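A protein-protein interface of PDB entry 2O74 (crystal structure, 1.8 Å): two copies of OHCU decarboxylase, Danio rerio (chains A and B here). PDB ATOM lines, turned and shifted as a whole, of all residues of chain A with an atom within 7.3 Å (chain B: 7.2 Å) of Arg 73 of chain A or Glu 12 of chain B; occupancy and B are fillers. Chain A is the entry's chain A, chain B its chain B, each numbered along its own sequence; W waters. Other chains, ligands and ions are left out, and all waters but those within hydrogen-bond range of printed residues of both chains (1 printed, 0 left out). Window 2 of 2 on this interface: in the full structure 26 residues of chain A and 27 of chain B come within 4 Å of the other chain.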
ATOM      1  N   ARG A  65      24.936  -2.986  23.667  1.00  0.00           N
ATOM      2  CA  ARG A  65      24.287  -1.773  23.193  1.00  0.00           C
ATOM      3  C   ARG A  65      24.951  -0.498  23.705  1.00  0.00           C
ATOM      4  O   ARG A  65      24.654   0.591  23.249  1.00  0.00           O
ATOM      5  CB  ARG A  65      22.820  -1.797  23.600  1.00  0.00           C
ATOM      6  CG  ARG A  65      21.986  -2.799  22.822  1.00  0.00           C
ATOM      7  CD  ARG A  65      20.608  -2.989  23.456  1.00  0.00           C
ATOM      8  NE  ARG A  65      20.015  -4.150  22.825  1.00  0.00           N
ATOM      9  CZ  ARG A  65      19.226  -5.040  23.396  1.00  0.00           C
ATOM     10  NH1 ARG A  65      18.843  -4.917  24.670  1.00  0.00           N
ATOM     11  NH2 ARG A  65      18.817  -6.076  22.665  1.00  0.00           N
ATOM     12  N   HIS A  67      28.169  -0.113  23.385  1.00  0.00           N
ATOM     13  CA  HIS A  67      29.376   0.004  22.547  1.00  0.00           C
ATOM     14  C   HIS A  67      29.035   0.771  21.262  1.00  0.00           C
ATOM     15  O   HIS A  67      27.928   0.631  20.725  1.00  0.00           O
ATOM     16  CB  HIS A  67      29.949  -1.374  22.195  1.00  0.00           C
ATOM     17  CG  HIS A  67      30.632  -2.069  23.338  1.00  0.00           C
ATOM     18  ND1 HIS A  67      29.947  -2.546  24.439  1.00  0.00           N
ATOM     19  CD2 HIS A  67      31.941  -2.359  23.548  1.00  0.00           C
ATOM     20  CE1 HIS A  67      30.810  -3.097  25.280  1.00  0.00           C
ATOM     21  NE2 HIS A  67      32.025  -3.003  24.760  1.00  0.00           N
ATOM     22  N   PRO A  68      29.970   1.601  20.776  1.00  0.00           N
ATOM     23  CA  PRO A  68      29.721   2.314  19.518  1.00  0.00           C
ATOM     24  C   PRO A  68      30.067   1.449  18.317  1.00  0.00           C
ATOM     25  O   PRO A  68      30.910   0.554  18.414  1.00  0.00           O
ATOM     26  CB  PRO A  68      30.670   3.510  19.604  1.00  0.00           C
ATOM     27  CG  PRO A  68      31.856   2.987  20.384  1.00  0.00           C
ATOM     28  CD  PRO A  68      31.270   1.975  21.381  1.00  0.00           C
ATOM     29  N   ASP A  69      29.422   1.705  17.183  1.00  0.00           N
ATOM     30  CA  ASP A  69      29.730   0.945  15.978  1.00  0.00           C
ATOM     31  C   ASP A  69      31.161   1.274  15.541  1.00  0.00           C
ATOM     32  O   ASP A  69      31.616   2.420  15.662  1.00  0.00           O
ATOM     33  CB  ASP A  69      28.799   1.333  14.823  1.00  0.00           C
ATOM     34  CG  ASP A  69      27.438   0.646  14.874  1.00  0.00           C
ATOM     35  OD1 ASP A  69      27.124  -0.106  15.832  1.00  0.00           O
ATOM     36  OD2 ASP A  69      26.678   0.857  13.903  1.00  0.00           O
ATOM     37  N   LEU A  70      31.859   0.261  15.059  1.00  0.00           N
ATOM     38  CA  LEU A  70      33.134   0.453  14.365  1.00  0.00           C
ATOM     39  C   LEU A  70      32.886   1.309  13.126  1.00  0.00           C
ATOM     40  O   LEU A  70      32.054   0.945  12.289  1.00  0.00           O
ATOM     41  CB  LEU A  70      33.693  -0.886  13.934  1.00  0.00           C
ATOM     42  CG  LEU A  70      34.148  -1.866  15.015  1.00  0.00           C
ATOM     43  CD1 LEU A  70      34.435  -3.195  14.360  1.00  0.00           C
ATOM     44  CD2 LEU A  70      35.361  -1.320  15.778  1.00  0.00           C
ATOM     45  N   ALA A  71      33.574   2.450  13.062  1.00  0.00           N
ATOM     46  CA  ALA A  71      33.532   3.398  11.940  1.00  0.00           C
ATOM     47  C   ALA A  71      32.230   4.194  11.839  1.00  0.00           C
ATOM     48  O   ALA A  71      31.960   4.853  10.824  1.00  0.00           O
ATOM     49  CB  ALA A  71      33.830   2.676  10.634  1.00  0.00           C
ATOM     50  N   GLY A  72      31.432   4.163  12.904  1.00  0.00           N
ATOM     51  CA  GLY A  72      30.090   4.725  12.838  1.00  0.00           C
ATOM     52  C   GLY A  72      29.986   6.192  13.181  1.00  0.00           C
ATOM     53  O   GLY A  72      30.969   6.934  13.137  1.00  0.00           O
ATOM     54  N   ARG A  73      28.777   6.617  13.528  1.00  0.00           N
ATOM     55  CA  ARG A  73      28.488   8.026  13.774  1.00  0.00           C
ATOM     56  C   ARG A  73      29.406   8.693  14.803  1.00  0.00           C
ATOM     57  O   ARG A  73      29.826   9.834  14.614  1.00  0.00           O
ATOM     58  CB  ARG A  73      27.019   8.186  14.190  1.00  0.00           C
ATOM     59  CG  ARG A  73      26.510   9.620  14.291  1.00  0.00           C
ATOM     60  CD  ARG A  73      25.083   9.622  14.841  1.00  0.00           C
ATOM     61  NE  ARG A  73      24.381   8.394  14.461  1.00  0.00           N
ATOM     62  CZ  ARG A  73      23.115   8.122  14.770  1.00  0.00           C
ATOM     63  NH1 ARG A  73      22.394   8.990  15.468  1.00  0.00           N
ATOM     64  NH2 ARG A  73      22.564   6.979  14.373  1.00  0.00           N
ATOM     65  N   ASP A  74      29.710   7.997  15.898  1.00  0.00           N
ATOM     66  CA  ASP A  74      30.515   8.611  16.956  1.00  0.00           C
ATOM     67  C   ASP A  74      31.969   8.792  16.531  1.00  0.00           C
ATOM     68  O   ASP A  74      32.581   9.816  16.830  1.00  0.00           O
ATOM     69  CB  ASP A  74      30.426   7.829  18.273  1.00  0.00           C
ATOM     70  CG  ASP A  74      29.042   7.910  18.910  1.00  0.00           C
ATOM     71  OD1 ASP A  74      28.108   8.456  18.276  1.00  0.00           O
ATOM     72  OD2 ASP A  74      28.878   7.416  20.041  1.00  0.00           O
ATOM     73  N   LEU A  75      32.518   7.794  15.855  1.00  0.00           N
ATOM     74  CA  LEU A  75      33.841   7.926  15.261  1.00  0.00           C
ATOM     75  C   LEU A  75      33.892   9.177  14.352  1.00  0.00           C
ATOM     76  O   LEU A  75      34.774  10.029  14.492  1.00  0.00           O
ATOM     77  CB  LEU A  75      34.203   6.656  14.480  1.00  0.00           C
ATOM     78  CG  LEU A  75      35.568   6.655  13.782  1.00  0.00           C
ATOM     79  CD1 LEU A  75      36.686   6.152  14.706  1.00  0.00           C
ATOM     80  CD2 LEU A  75      35.508   5.823  12.512  1.00  0.00           C
ATOM     81  N   GLN A  76      32.922   9.304  13.454  1.00  0.00           N
ATOM     82  CA  GLN A  76      32.896  10.417  12.499  1.00  0.00           C
ATOM     83  C   GLN A  76      32.757  11.773  13.177  1.00  0.00           C
ATOM     84  O   GLN A  76      33.338  12.761  12.724  1.00  0.00           O
ATOM     85  CB  GLN A  76      31.763  10.233  11.482  1.00  0.00           C
ATOM     86  CG  GLN A  76      31.723   8.869  10.809  1.00  0.00           C
ATOM     87  CD  GLN A  76      33.022   8.515  10.129  1.00  0.00           C
ATOM     88  OE1 GLN A  76      33.807   9.395   9.761  1.00  0.00           O
ATOM     89  NE2 GLN A  76      33.261   7.223   9.950  1.00  0.00           N
ATOM     90  N   SER A  77      31.986  11.814  14.262  1.00  0.00           N
ATOM     91  CA  SER A  77      31.704  13.056  14.965  1.00  0.00           C
ATOM     92  C   SER A  77      32.818  13.398  15.956  1.00  0.00           C
ATOM     93  O   SER A  77      32.819  14.478  16.562  1.00  0.00           O
ATOM     94  CB  SER A  77      30.351  12.955  15.679  1.00  0.00           C
ATOM     95  OG  SER A  77      29.793  14.238  15.928  1.00  0.00           O
ATOM     96  N   GLY A  78      33.773  12.480  16.095  1.00  0.00           N
ATOM     97  CA  GLY A  78      34.877  12.645  17.042  1.00  0.00           C
ATOM     98  C   GLY A  78      34.407  12.556  18.482  1.00  0.00           C
ATOM     99  O   GLY A  78      34.936  13.237  19.368  1.00  0.00           O
ATOM    100  N   THR A  79      33.406  11.715  18.728  1.00  0.00           N
ATOM    101  CA  THR A  79      32.792  11.663  20.054  1.00  0.00           C
ATOM    102  C   THR A  79      32.890  10.277  20.685  1.00  0.00           C
ATOM    103  O   THR A  79      32.040   9.905  21.492  1.00  0.00           O
ATOM    104  CB  THR A  79      31.308  12.101  20.021  1.00  0.00           C
ATOM    105  OG1 THR A  79      30.589  11.281  19.087  1.00  0.00           O
ATOM    106  CG2 THR A  79      31.171  13.576  19.630  1.00  0.00           C
ATOM    107  N   LEU A  80      33.909   9.509  20.305  1.00  0.00           N
ATOM    108  CA  LEU A  80      34.178   8.223  20.954  1.00  0.00           C
ATOM    109  C   LEU A  80      34.880   8.447  22.281  1.00  0.00           C
ATOM    110  O   LEU A  80      35.536   9.482  22.488  1.00  0.00           O
ATOM    111  CB  LEU A  80      35.064   7.316  20.091  1.00  0.00           C
ATOM    112  CG  LEU A  80      34.734   7.010  18.632  1.00  0.00           C
ATOM    113  CD1 LEU A  80      35.180   8.172  17.799  1.00  0.00           C
ATOM    114  CD2 LEU A  80      35.433   5.758  18.135  1.00  0.00           C
ATOM    115  N   TYR A 105      29.070   1.038   7.375  1.00  0.00           N
ATOM    116  CA  TYR A 105      27.688   1.329   7.737  1.00  0.00           C
ATOM    117  C   TYR A 105      26.733   0.178   7.375  1.00  0.00           C
ATOM    118  O   TYR A 105      25.895  -0.217   8.195  1.00  0.00           O
ATOM    119  CB  TYR A 105      27.231   2.676   7.148  1.00  0.00           C
ATOM    120  CG  TYR A 105      25.886   3.119   7.687  1.00  0.00           C
ATOM    121  CD1 TYR A 105      25.795   3.886   8.849  1.00  0.00           C
ATOM    122  CD2 TYR A 105      24.708   2.744   7.051  1.00  0.00           C
ATOM    123  CE1 TYR A 105      24.557   4.273   9.360  1.00  0.00           C
ATOM    124  CE2 TYR A 105      23.473   3.123   7.549  1.00  0.00           C
ATOM    125  CZ  TYR A 105      23.402   3.884   8.700  1.00  0.00           C
ATOM    126  OH  TYR A 105      22.161   4.251   9.188  1.00  0.00           O
ATOM    127  N   ASN A 108      27.288  -3.246   9.346  1.00  0.00           N
ATOM    128  CA  ASN A 108      26.774  -2.962  10.694  1.00  0.00           C
ATOM    129  C   ASN A 108      25.249  -2.888  10.747  1.00  0.00           C
ATOM    130  O   ASN A 108      24.626  -3.417  11.668  1.00  0.00           O
ATOM    131  CB  ASN A 108      27.374  -1.677  11.241  1.00  0.00           C
ATOM    132  CG  ASN A 108      28.690  -1.916  11.952  1.00  0.00           C
ATOM    133  OD1 ASN A 108      28.856  -2.926  12.644  1.00  0.00           O
ATOM    134  ND2 ASN A 108      29.632  -0.982  11.791  1.00  0.00           N
ATOM    135  N   LYS A 112      23.131  -5.474  13.125  1.00  0.00           N
ATOM    136  CA  LYS A 112      22.308  -4.978  14.228  1.00  0.00           C
ATOM    137  C   LYS A 112      20.815  -5.241  14.001  1.00  0.00           C
ATOM    138  O   LYS A 112      20.067  -5.441  14.952  1.00  0.00           O
ATOM    139  CB  LYS A 112      22.610  -3.498  14.533  1.00  0.00           C
ATOM    140  CG  LYS A 112      21.961  -2.503  13.594  1.00  0.00           C
ATOM    141  CD  LYS A 112      22.257  -1.030  13.965  1.00  0.00           C
ATOM    142  CE  LYS A 112      23.748  -0.665  13.842  1.00  0.00           C
ATOM    143  NZ  LYS A 112      23.955   0.819  13.951  1.00  0.00           N
ATOM    144  N   PHE A 117      21.736  -5.763  18.600  1.00  0.00           N
ATOM    145  CA  PHE A 117      22.803  -5.075  19.325  1.00  0.00           C
ATOM    146  C   PHE A 117      23.969  -4.859  18.356  1.00  0.00           C
ATOM    147  O   PHE A 117      23.990  -5.466  17.283  1.00  0.00           O
ATOM    148  CB  PHE A 117      23.232  -5.851  20.587  1.00  0.00           C
ATOM    149  CG  PHE A 117      23.438  -7.343  20.378  1.00  0.00           C
ATOM    150  CD1 PHE A 117      22.518  -8.262  20.880  1.00  0.00           C
ATOM    151  CD2 PHE A 117      24.570  -7.822  19.717  1.00  0.00           C
ATOM    152  CE1 PHE A 117      22.705  -9.647  20.723  1.00  0.00           C
ATOM    153  CE2 PHE A 117      24.772  -9.188  19.540  1.00  0.00           C
ATOM    154  CZ  PHE A 117      23.840 -10.111  20.049  1.00  0.00           C
ATOM    155  N   PRO A 118      24.921  -3.986  18.712  1.00  0.00           N
ATOM    156  CA  PRO A 118      26.026  -3.683  17.784  1.00  0.00           C
ATOM    157  C   PRO A 118      27.002  -4.816  17.610  1.00  0.00           C
ATOM    158  O   PRO A 118      27.181  -5.645  18.507  1.00  0.00           O
ATOM    159  CB  PRO A 118      26.740  -2.515  18.462  1.00  0.00           C
ATOM    160  CG  PRO A 118      25.746  -1.963  19.461  1.00  0.00           C
ATOM    161  CD  PRO A 118      25.014  -3.175  19.939  1.00  0.00           C
ATOM    162  N   LEU B   9      11.290   2.687  18.377  1.00  0.00           N
ATOM    163  CA  LEU B   9      12.653   3.221  18.436  1.00  0.00           C
ATOM    164  C   LEU B   9      13.695   2.124  18.175  1.00  0.00           C
ATOM    165  O   LEU B   9      13.605   1.023  18.731  1.00  0.00           O
ATOM    166  CB  LEU B   9      12.911   3.860  19.807  1.00  0.00           C
ATOM    167  CG  LEU B   9      12.901   5.373  20.139  1.00  0.00           C
ATOM    168  CD1 LEU B   9      12.323   6.309  19.088  1.00  0.00           C
ATOM    169  CD2 LEU B   9      12.296   5.643  21.526  1.00  0.00           C
ATOM    170  N   ALA B  10      14.689   2.439  17.346  1.00  0.00           N
ATOM    171  CA  ALA B  10      15.902   1.627  17.236  1.00  0.00           C
ATOM    172  C   ALA B  10      16.601   1.653  18.594  1.00  0.00           C
ATOM    173  O   ALA B  10      16.485   2.644  19.320  1.00  0.00           O
ATOM    174  CB  ALA B  10      16.823   2.213  16.180  1.00  0.00           C
ATOM    175  N   TYR B  11      17.351   0.605  18.929  1.00  0.00           N
ATOM    176  CA  TYR B  11      17.966   0.565  20.261  1.00  0.00           C
ATOM    177  C   TYR B  11      18.894   1.763  20.488  1.00  0.00           C
ATOM    178  O   TYR B  11      18.983   2.268  21.606  1.00  0.00           O
ATOM    179  CB  TYR B  11      18.664  -0.768  20.562  1.00  0.00           C
ATOM    180  CG  TYR B  11      19.901  -1.045  19.737  1.00  0.00           C
ATOM    181  CD1 TYR B  11      19.867  -1.981  18.714  1.00  0.00           C
ATOM    182  CD2 TYR B  11      21.109  -0.375  19.989  1.00  0.00           C
ATOM    183  CE1 TYR B  11      20.999  -2.243  17.944  1.00  0.00           C
ATOM    184  CE2 TYR B  11      22.257  -0.634  19.216  1.00  0.00           C
ATOM    185  CZ  TYR B  11      22.175  -1.576  18.191  1.00  0.00           C
ATOM    186  OH  TYR B  11      23.277  -1.865  17.402  1.00  0.00           O
ATOM    187  N   GLU B  12      19.586   2.221  19.441  1.00  0.00           N
ATOM    188  CA  GLU B  12      20.480   3.370  19.611  1.00  0.00           C
ATOM    189  C   GLU B  12      19.740   4.607  20.111  1.00  0.00           C
ATOM    190  O   GLU B  12      20.252   5.348  20.942  1.00  0.00           O
ATOM    191  CB  GLU B  12      21.229   3.693  18.321  1.00  0.00           C
ATOM    192  CG  GLU B  12      22.325   2.712  18.007  1.00  0.00           C
ATOM    193  CD  GLU B  12      22.715   2.764  16.555  1.00  0.00           C
ATOM    194  OE1 GLU B  12      23.263   3.805  16.152  1.00  0.00           O
ATOM    195  OE2 GLU B  12      22.451   1.780  15.823  1.00  0.00           O
ATOM    196  N   ASP B  13      18.527   4.816  19.610  1.00  0.00           N
ATOM    197  CA  ASP B  13      17.753   6.001  19.969  1.00  0.00           C
ATOM    198  C   ASP B  13      17.071   5.836  21.312  1.00  0.00           C
ATOM    199  O   ASP B  13      16.940   6.803  22.069  1.00  0.00           O
ATOM    200  CB  ASP B  13      16.713   6.299  18.901  1.00  0.00           C
ATOM    201  CG  ASP B  13      17.332   6.813  17.626  1.00  0.00           C
ATOM    202  OD1 ASP B  13      18.433   7.400  17.686  1.00  0.00           O
ATOM    203  OD2 ASP B  13      16.725   6.625  16.554  1.00  0.00           O
ATOM    204  N   PHE B  14      16.606   4.616  21.575  1.00  0.00           N
ATOM    205  CA  PHE B  14      16.064   4.248  22.887  1.00  0.00           C
ATOM    206  C   PHE B  14      17.120   4.489  23.969  1.00  0.00           C
ATOM    207  O   PHE B  14      16.819   5.078  25.003  1.00  0.00           O
ATOM    208  CB  PHE B  14      15.640   2.776  22.888  1.00  0.00           C
ATOM    209  CG  PHE B  14      14.885   2.357  24.116  1.00  0.00           C
ATOM    210  CD1 PHE B  14      15.557   1.875  25.234  1.00  0.00           C
ATOM    211  CD2 PHE B  14      13.499   2.454  24.160  1.00  0.00           C
ATOM    212  CE1 PHE B  14      14.851   1.470  26.368  1.00  0.00           C
ATOM    213  CE2 PHE B  14      12.787   2.055  25.287  1.00  0.00           C
ATOM    214  CZ  PHE B  14      13.462   1.575  26.397  1.00  0.00           C
ATOM    215  N   VAL B  15      18.361   4.060  23.717  1.00  0.00           N
ATOM    216  CA  VAL B  15      19.458   4.282  24.678  1.00  0.00           C
ATOM    217  C   VAL B  15      19.783   5.778  24.845  1.00  0.00           C
ATOM    218  O   VAL B  15      20.032   6.250  25.961  1.00  0.00           O
ATOM    219  CB  VAL B  15      20.743   3.486  24.314  1.00  0.00           C
ATOM    220  CG1 VAL B  15      21.863   3.760  25.354  1.00  0.00           C
ATOM    221  CG2 VAL B  15      20.447   1.996  24.270  1.00  0.00           C
ATOM    222  N   LYS B  16      19.763   6.533  23.751  1.00  0.00           N
ATOM    223  CA  LYS B  16      19.994   7.978  23.858  1.00  0.00           C
ATOM    224  C   LYS B  16      18.895   8.685  24.666  1.00  0.00           C
ATOM    225  O   LYS B  16      19.185   9.550  25.498  1.00  0.00           O
ATOM    226  CB  LYS B  16      20.214   8.612  22.470  1.00  0.00           C
ATOM    227  CG  LYS B  16      21.538   8.158  21.834  1.00  0.00           C
ATOM    228  CD  LYS B  16      21.970   9.001  20.635  1.00  0.00           C
ATOM    229  CE  LYS B  16      21.334   8.526  19.345  1.00  0.00           C
ATOM    230  NZ  LYS B  16      21.647   9.471  18.235  1.00  0.00           N
ATOM    231  N   LEU B  17      17.649   8.273  24.456  1.00  0.00           N
ATOM    232  CA  LEU B  17      16.489   8.865  25.138  1.00  0.00           C
ATOM    233  C   LEU B  17      16.424   8.508  26.619  1.00  0.00           C
ATOM    234  O   LEU B  17      16.202   9.374  27.462  1.00  0.00           O
ATOM    235  CB  LEU B  17      15.189   8.415  24.467  1.00  0.00           C
ATOM    236  CG  LEU B  17      13.909   9.115  24.948  1.00  0.00           C
ATOM    237  CD1 LEU B  17      14.041  10.634  24.770  1.00  0.00           C
ATOM    238  CD2 LEU B  17      12.709   8.599  24.176  1.00  0.00           C
ATOM    239  N   TRP B  33      15.193  -2.632  26.612  1.00  0.00           N
ATOM    240  CA  TRP B  33      14.741  -2.550  25.220  1.00  0.00           C
ATOM    241  C   TRP B  33      14.466  -3.948  24.667  1.00  0.00           C
ATOM    242  O   TRP B  33      13.647  -4.111  23.771  1.00  0.00           O
ATOM    243  CB  TRP B  33      15.786  -1.840  24.347  1.00  0.00           C
ATOM    244  CG  TRP B  33      15.393  -1.603  22.920  1.00  0.00           C
ATOM    245  CD1 TRP B  33      14.607  -0.592  22.435  1.00  0.00           C
ATOM    246  CD2 TRP B  33      15.801  -2.374  21.775  1.00  0.00           C
ATOM    247  NE1 TRP B  33      14.498  -0.695  21.065  1.00  0.00           N
ATOM    248  CE2 TRP B  33      15.214  -1.784  20.641  1.00  0.00           C
ATOM    249  CE3 TRP B  33      16.591  -3.521  21.610  1.00  0.00           C
ATOM    250  CZ2 TRP B  33      15.396  -2.293  19.354  1.00  0.00           C
ATOM    251  CZ3 TRP B  33      16.778  -4.025  20.326  1.00  0.00           C
ATOM    252  CH2 TRP B  33      16.173  -3.415  19.220  1.00  0.00           C
HETATM  253  O   HOH W   1      23.737   4.415  13.371  1.00  0.00           O
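The side-chain carboxylate (OE1) of Glu 12 of chain B lies within salt-bridge range of the guanidinium group (NH2) of Arg 73 of chain A, 3.7 Å away.
OE2 of Glu 12 of chain B is in salt-bridge range of NZ of Lys 112 of chain A (2.6 Å).
The side-chain amino group of Lys 16 of chain B sits close to the guanidinium group of Arg 73 of chain A, 2.9 Å away.
The side-chain hydroxyl (OH) of Tyr 11 of chain B lies close to the backbone nitrogen (N) of Pro 118 of chain A.
The side-chain carboxylate (OD2) of Asp 69 of chain A lies within salt-bridge range of the side-chain amino group (NZ) of Lys 112 of chain A, 2.7 Å away.
The indole nitrogen of Trp 33 of chain B lies within hydrogen-bond range of the backbone carbonyl oxygen of Leu 9 of chain B, at 3.0 Å.
The side-chain amino group (NZ) of Lys 16 of chain B lies within salt-bridge range of the side-chain carboxylate (OD1) of Asp 13 of chain B (3.9 Å).
Among the printed residues, merely in contact across the chains: Phe 117 of chain A with Tyr 11 of chain B, Lys 112 of chain A with Tyr 11 of chain B, Arg 65 of chain A with Trp 33 of chain B and Arg 65 of chain A with Tyr 11 of chain B.
Of the printed residues of chain A, Glu 12 of chain B touches Arg 73 (3.7 Å) and Lys 112 (2.6 Å).
Of the printed residues of chain A, Lys 16 of chain B touches Arg 73 (2.9 Å).
Printed residues of chain A within 4 Å of Trp 33 of chain B: Arg 65 (3.5 Å).
Of the printed residues of chain B, Pro 118 of chain A touches Tyr 11.
Ser 77 of chain A touches none of the printed residues of chain B.
The nearest residue of chain B that does not touch Arg 73 of chain A is Asp 13 of chain B (4.8 Å).
Of the 20 printed residues of chain A, 5 touch a printed residue of chain B.
Printed residues of chain A that touch a printed residue of chain B: Arg 65, Arg 73, Lys 112, Phe 117 and Pro 118.
Of the 10 printed residues of chain B, 4 touch a printed residue of chain A.
Among the printed residues, Asp or Glu carboxylates within 4 Å of a Lys or Arg side-chain nitrogen of the other chain: Arg 73 of chain A with Glu 12 of chain B and Lys 112 of chain A with Glu 12 of chain B.
No position is printed for both chains.
Of the 8 pairs that touch across the chains among the printed residues, none has its exchanged pair printed and touching as well.
Water W1 bridges OE1 of Glu 12 of chain B (2.9 Å) and NH2 of Arg 73 of chain A (3.0 Å).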
